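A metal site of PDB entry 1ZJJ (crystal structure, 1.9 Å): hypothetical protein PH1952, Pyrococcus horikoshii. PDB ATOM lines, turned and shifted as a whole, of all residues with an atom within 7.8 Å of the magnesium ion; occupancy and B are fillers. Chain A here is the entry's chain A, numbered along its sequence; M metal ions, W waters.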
ATOM      1  N   PHE A   6      15.352 -23.866 -14.403  1.00  0.00           N
ATOM      2  CA  PHE A   6      16.785 -24.073 -14.234  1.00  0.00           C
ATOM      3  C   PHE A   6      17.660 -23.172 -15.060  1.00  0.00           C
ATOM      4  O   PHE A   6      17.459 -23.039 -16.274  1.00  0.00           O
ATOM      5  CB  PHE A   6      17.211 -25.484 -14.628  1.00  0.00           C
ATOM      6  CG  PHE A   6      16.544 -26.582 -13.872  1.00  0.00           C
ATOM      7  CD1 PHE A   6      15.317 -27.076 -14.285  1.00  0.00           C
ATOM      8  CD2 PHE A   6      17.178 -27.176 -12.771  1.00  0.00           C
ATOM      9  CE1 PHE A   6      14.728 -28.155 -13.634  1.00  0.00           C
ATOM     10  CE2 PHE A   6      16.598 -28.256 -12.116  1.00  0.00           C
ATOM     11  CZ  PHE A   6      15.367 -28.749 -12.547  1.00  0.00           C
ATOM     12  N   ASP A   7      18.638 -22.563 -14.415  1.00  0.00           N
ATOM     13  CA  ASP A   7      19.611 -21.782 -15.136  1.00  0.00           C
ATOM     14  C   ASP A   7      20.426 -22.950 -15.713  1.00  0.00           C
ATOM     15  O   ASP A   7      20.371 -24.062 -15.177  1.00  0.00           O
ATOM     16  CB  ASP A   7      20.471 -20.963 -14.191  1.00  0.00           C
ATOM     17  CG  ASP A   7      21.769 -20.560 -14.828  1.00  0.00           C
ATOM     18  OD1 ASP A   7      21.748 -19.820 -15.832  1.00  0.00           O
ATOM     19  OD2 ASP A   7      22.804 -21.007 -14.326  1.00  0.00           O
ATOM     20  N   MET A   8      21.198 -22.716 -16.765  1.00  0.00           N
ATOM     21  CA  MET A   8      21.912 -23.827 -17.373  1.00  0.00           C
ATOM     22  C   MET A   8      23.398 -24.035 -17.045  1.00  0.00           C
ATOM     23  O   MET A   8      23.754 -25.039 -16.430  1.00  0.00           O
ATOM     24  CB  MET A   8      21.720 -23.762 -18.886  1.00  0.00           C
ATOM     25  CG  MET A   8      20.264 -23.606 -19.297  1.00  0.00           C
ATOM     26  SD  MET A   8      20.015 -23.489 -21.078  1.00  0.00           S
ATOM     27  CE  MET A   8      20.138 -25.154 -21.474  1.00  0.00           C
ATOM     28  N   ASP A   9      24.247 -23.108 -17.464  1.00  0.00           N
ATOM     29  CA  ASP A   9      25.680 -23.238 -17.200  1.00  0.00           C
ATOM     30  C   ASP A   9      25.975 -23.199 -15.707  1.00  0.00           C
ATOM     31  O   ASP A   9      25.583 -22.267 -15.020  1.00  0.00           O
ATOM     32  CB  ASP A   9      26.431 -22.119 -17.919  1.00  0.00           C
ATOM     33  CG  ASP A   9      27.921 -22.385 -18.030  1.00  0.00           C
ATOM     34  OD1 ASP A   9      28.357 -23.524 -17.742  1.00  0.00           O
ATOM     35  OD2 ASP A   9      28.660 -21.455 -18.419  1.00  0.00           O
ATOM     36  N   GLY A  10      26.654 -24.219 -15.195  1.00  0.00           N
ATOM     37  CA  GLY A  10      26.975 -24.268 -13.780  1.00  0.00           C
ATOM     38  C   GLY A  10      25.902 -24.952 -12.957  1.00  0.00           C
ATOM     39  O   GLY A  10      26.036 -25.097 -11.741  1.00  0.00           O
ATOM     40  N   VAL A  11      24.835 -25.386 -13.614  1.00  0.00           N
ATOM     41  CA  VAL A  11      23.729 -26.042 -12.941  1.00  0.00           C
ATOM     42  C   VAL A  11      23.445 -27.406 -13.576  1.00  0.00           C
ATOM     43  O   VAL A  11      23.448 -28.432 -12.903  1.00  0.00           O
ATOM     44  CB  VAL A  11      22.447 -25.168 -13.023  1.00  0.00           C
ATOM     45  CG1 VAL A  11      21.267 -25.907 -12.424  1.00  0.00           C
ATOM     46  CG2 VAL A  11      22.683 -23.846 -12.280  1.00  0.00           C
ATOM     47  N   LEU A  12      23.217 -27.405 -14.885  1.00  0.00           N
ATOM     48  CA  LEU A  12      22.938 -28.641 -15.611  1.00  0.00           C
ATOM     49  C   LEU A  12      24.232 -29.225 -16.152  1.00  0.00           C
ATOM     50  O   LEU A  12      24.336 -30.418 -16.407  1.00  0.00           O
ATOM     51  CB  LEU A  12      21.961 -28.359 -16.758  1.00  0.00           C
ATOM     52  CG  LEU A  12      20.625 -27.754 -16.348  1.00  0.00           C
ATOM     53  CD1 LEU A  12      19.807 -27.417 -17.579  1.00  0.00           C
ATOM     54  CD2 LEU A  12      19.861 -28.722 -15.464  1.00  0.00           C
ATOM     55  N   TYR A  13      25.226 -28.367 -16.331  1.00  0.00           N
ATOM     56  CA  TYR A  13      26.518 -28.785 -16.833  1.00  0.00           C
ATOM     57  C   TYR A  13      27.535 -27.681 -16.627  1.00  0.00           C
ATOM     58  O   TYR A  13      27.208 -26.596 -16.119  1.00  0.00           O
ATOM     59  CB  TYR A  13      26.433 -29.096 -18.338  1.00  0.00           C
ATOM     60  CG  TYR A  13      25.930 -27.933 -19.167  1.00  0.00           C
ATOM     61  CD1 TYR A  13      26.708 -26.806 -19.375  1.00  0.00           C
ATOM     62  CD2 TYR A  13      24.654 -27.965 -19.736  1.00  0.00           C
ATOM     63  CE1 TYR A  13      26.232 -25.728 -20.128  1.00  0.00           C
ATOM     64  CE2 TYR A  13      24.165 -26.894 -20.487  1.00  0.00           C
ATOM     65  CZ  TYR A  13      24.959 -25.776 -20.681  1.00  0.00           C
ATOM     66  OH  TYR A  13      24.504 -24.715 -21.411  1.00  0.00           O
ATOM     67  N   LEU A  39      16.527 -21.804 -18.461  1.00  0.00           N
ATOM     68  CA  LEU A  39      16.642 -20.372 -18.685  1.00  0.00           C
ATOM     69  C   LEU A  39      18.103 -19.983 -18.802  1.00  0.00           C
ATOM     70  O   LEU A  39      18.913 -20.354 -17.952  1.00  0.00           O
ATOM     71  CB  LEU A  39      15.991 -19.657 -17.497  1.00  0.00           C
ATOM     72  CG  LEU A  39      15.495 -18.217 -17.608  1.00  0.00           C
ATOM     73  CD1 LEU A  39      14.303 -18.161 -18.544  1.00  0.00           C
ATOM     74  CD2 LEU A  39      15.103 -17.723 -16.224  1.00  0.00           C
ATOM     75  N   THR A  40      18.427 -19.249 -19.853  1.00  0.00           N
ATOM     76  CA  THR A  40      19.803 -18.787 -20.039  1.00  0.00           C
ATOM     77  C   THR A  40      19.819 -17.361 -20.573  1.00  0.00           C
ATOM     78  O   THR A  40      19.024 -17.011 -21.440  1.00  0.00           O
ATOM     79  CB  THR A  40      20.588 -19.672 -21.035  1.00  0.00           C
ATOM     80  OG1 THR A  40      21.917 -19.154 -21.176  1.00  0.00           O
ATOM     81  CG2 THR A  40      19.904 -19.687 -22.398  1.00  0.00           C
ATOM     82  N   ASP A 154      24.837  -9.403 -18.004  1.00  0.00           N
ATOM     83  CA  ASP A 154      26.121 -10.077 -17.856  1.00  0.00           C
ATOM     84  C   ASP A 154      27.344  -9.318 -18.374  1.00  0.00           C
ATOM     85  O   ASP A 154      27.504  -9.111 -19.578  1.00  0.00           O
ATOM     86  CB  ASP A 154      26.046 -11.457 -18.504  1.00  0.00           C
ATOM     87  CG  ASP A 154      24.997 -12.349 -17.858  1.00  0.00           C
ATOM     88  OD1 ASP A 154      25.324 -13.046 -16.877  1.00  0.00           O
ATOM     89  OD2 ASP A 154      23.834 -12.331 -18.323  1.00  0.00           O
ATOM     90  N   LYS A 187      17.686 -12.147 -16.742  1.00  0.00           N
ATOM     91  CA  LYS A 187      17.749 -12.124 -15.270  1.00  0.00           C
ATOM     92  C   LYS A 187      18.896 -11.279 -14.747  1.00  0.00           C
ATOM     93  O   LYS A 187      19.982 -11.284 -15.297  1.00  0.00           O
ATOM     94  CB  LYS A 187      17.871 -13.544 -14.723  1.00  0.00           C
ATOM     95  CG  LYS A 187      18.661 -14.549 -15.547  1.00  0.00           C
ATOM     96  CD  LYS A 187      18.290 -15.970 -15.123  1.00  0.00           C
ATOM     97  CE  LYS A 187      18.939 -17.043 -15.987  1.00  0.00           C
ATOM     98  NZ  LYS A 187      20.351 -17.314 -15.624  1.00  0.00           N
ATOM     99  N   VAL A 208      16.381 -22.411  -9.894  1.00  0.00           N
ATOM    100  CA  VAL A 208      17.626 -23.093  -9.524  1.00  0.00           C
ATOM    101  C   VAL A 208      18.784 -22.494 -10.309  1.00  0.00           C
ATOM    102  O   VAL A 208      18.803 -22.534 -11.540  1.00  0.00           O
ATOM    103  CB  VAL A 208      17.539 -24.613  -9.831  1.00  0.00           C
ATOM    104  CG1 VAL A 208      18.782 -25.326  -9.334  1.00  0.00           C
ATOM    105  CG2 VAL A 208      16.306 -25.205  -9.178  1.00  0.00           C
ATOM    106  N   GLY A 209      19.751 -21.918  -9.593  1.00  0.00           N
ATOM    107  CA  GLY A 209      20.889 -21.314 -10.248  1.00  0.00           C
ATOM    108  C   GLY A 209      22.176 -21.359  -9.434  1.00  0.00           C
ATOM    109  O   GLY A 209      22.157 -21.748  -8.265  1.00  0.00           O
ATOM    110  N   ASP A 210      23.290 -20.956 -10.048  1.00  0.00           N
ATOM    111  CA  ASP A 210      24.585 -20.954  -9.373  1.00  0.00           C
ATOM    112  C   ASP A 210      25.148 -19.551  -9.165  1.00  0.00           C
ATOM    113  O   ASP A 210      26.219 -19.403  -8.576  1.00  0.00           O
ATOM    114  CB  ASP A 210      25.597 -21.760 -10.169  1.00  0.00           C
ATOM    115  CG  ASP A 210      25.875 -21.143 -11.523  1.00  0.00           C
ATOM    116  OD1 ASP A 210      24.908 -20.929 -12.263  1.00  0.00           O
ATOM    117  OD2 ASP A 210      27.054 -20.872 -11.849  1.00  0.00           O
ATOM    118  N   ARG A 211      24.448 -18.532  -9.654  1.00  0.00           N
ATOM    119  CA  ARG A 211      24.929 -17.156  -9.489  1.00  0.00           C
ATOM    120  C   ARG A 211      24.017 -16.367  -8.545  1.00  0.00           C
ATOM    121  O   ARG A 211      22.822 -16.207  -8.800  1.00  0.00           O
ATOM    122  CB  ARG A 211      24.986 -16.428 -10.837  1.00  0.00           C
ATOM    123  CG  ARG A 211      26.073 -16.899 -11.797  1.00  0.00           C
ATOM    124  CD  ARG A 211      25.983 -16.137 -13.128  1.00  0.00           C
ATOM    125  NE  ARG A 211      26.803 -16.742 -14.177  1.00  0.00           N
ATOM    126  CZ  ARG A 211      28.049 -16.363 -14.485  1.00  0.00           C
ATOM    127  NH1 ARG A 211      28.623 -15.373 -13.811  1.00  0.00           N
ATOM    128  NH2 ARG A 211      28.703 -16.981 -15.451  1.00  0.00           N
ATOM    129  N   THR A 214      22.667 -12.989 -10.080  1.00  0.00           N
ATOM    130  CA  THR A 214      21.666 -13.030 -11.156  1.00  0.00           C
ATOM    131  C   THR A 214      20.511 -13.997 -10.844  1.00  0.00           C
ATOM    132  O   THR A 214      19.358 -13.571 -10.728  1.00  0.00           O
ATOM    133  CB  THR A 214      22.288 -13.371 -12.565  1.00  0.00           C
ATOM    134  OG1 THR A 214      22.407 -14.785 -12.718  1.00  0.00           O
ATOM    135  CG2 THR A 214      23.678 -12.713 -12.719  1.00  0.00           C
ATOM    136  N   ASP A 215      20.810 -15.288 -10.699  1.00  0.00           N
ATOM    137  CA  ASP A 215      19.746 -16.256 -10.426  1.00  0.00           C
ATOM    138  C   ASP A 215      19.022 -16.068  -9.091  1.00  0.00           C
ATOM    139  O   ASP A 215      17.788 -16.072  -9.049  1.00  0.00           O
ATOM    140  CB  ASP A 215      20.280 -17.685 -10.482  1.00  0.00           C
ATOM    141  CG  ASP A 215      20.989 -17.991 -11.753  1.00  0.00           C
ATOM    142  OD1 ASP A 215      20.417 -17.763 -12.841  1.00  0.00           O
ATOM    143  OD2 ASP A 215      22.142 -18.462 -11.671  1.00  0.00           O
ATOM    144  N   VAL A 229      22.798 -23.781  -6.114  1.00  0.00           N
ATOM    145  CA  VAL A 229      23.584 -25.011  -6.162  1.00  0.00           C
ATOM    146  C   VAL A 229      25.031 -24.571  -6.104  1.00  0.00           C
ATOM    147  O   VAL A 229      25.352 -23.430  -6.465  1.00  0.00           O
ATOM    148  CB  VAL A 229      23.324 -25.834  -7.454  1.00  0.00           C
ATOM    149  CG1 VAL A 229      21.879 -26.364  -7.454  1.00  0.00           C
ATOM    150  CG2 VAL A 229      23.586 -24.955  -8.692  1.00  0.00           C
ATOM    151  N   GLY A 232      28.547 -24.292  -9.519  1.00  0.00           N
ATOM    152  CA  GLY A 232      28.939 -23.232 -10.430  1.00  0.00           C
ATOM    153  C   GLY A 232      29.734 -22.076  -9.838  1.00  0.00           C
ATOM    154  O   GLY A 232      30.631 -22.257  -9.026  1.00  0.00           O
ATOM    155  N   VAL A 233      29.371 -20.860 -10.260  1.00  0.00           N
ATOM    156  CA  VAL A 233      30.053 -19.650  -9.828  1.00  0.00           C
ATOM    157  C   VAL A 233      30.066 -19.314  -8.328  1.00  0.00           C
ATOM    158  O   VAL A 233      31.133 -19.116  -7.746  1.00  0.00           O
ATOM    159  CB  VAL A 233      29.495 -18.426 -10.592  1.00  0.00           C
ATOM    160  CG1 VAL A 233      30.177 -17.141 -10.117  1.00  0.00           C
ATOM    161  CG2 VAL A 233      29.718 -18.625 -12.084  1.00  0.00           C
HETATM  162 MG    MG M   1      24.828 -20.333 -14.382  1.00  0.00          MG
HETATM  163  O   HOH W   1      23.947 -18.475 -13.587  1.00  0.00           O
HETATM  164  O   HOH W   2      26.752 -19.653 -14.249  1.00  0.00           O
HETATM  165  O   HOH W   3      24.653 -19.529 -16.361  1.00  0.00           O
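The backbone NH of Asp 7 is in hydrogen-bond range of the backbone carbonyl oxygen of Val 208 (2.9 Å). The side-chain carboxylate (OD2) of Asp 210 is in hydrogen-bond range of the backbone NH (N) of Val 233, 2.8 Å away. The backbone NH (N) of Asp 210 lies within hydrogen-bond range of the side-chain carboxylate (OD2) of Asp 215, at 3.2 Å. NZ of Lys 187 is in salt-bridge range of OD1 of Asp 7 (2.9 Å).
Along chain A the residues within 4 Å of the magnesium ion span positions 7 to 210. The nearest printed residue that does not touch the magnesium ion is Arg 211 (4.1 Å).
The magnesium ion is bound by water W2 (2.0 Å), OD2 of Asp 7 (2.1 Å), water W3 (2.1 Å), O of Asp 9 (2.2 Å), OD1 of Asp 210 (2.2 Å) and water W1 (2.2 Å). The magnesium ion has six donor atoms within binding distance.
Water W1 lies within hydrogen-bond range of OD2 of Asp 215, NE of Arg 211 and OD1 of Asp 7. Water W2 bridges OD2 of Asp 210 (2.7 Å) and NE of Arg 211 (2.9 Å).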
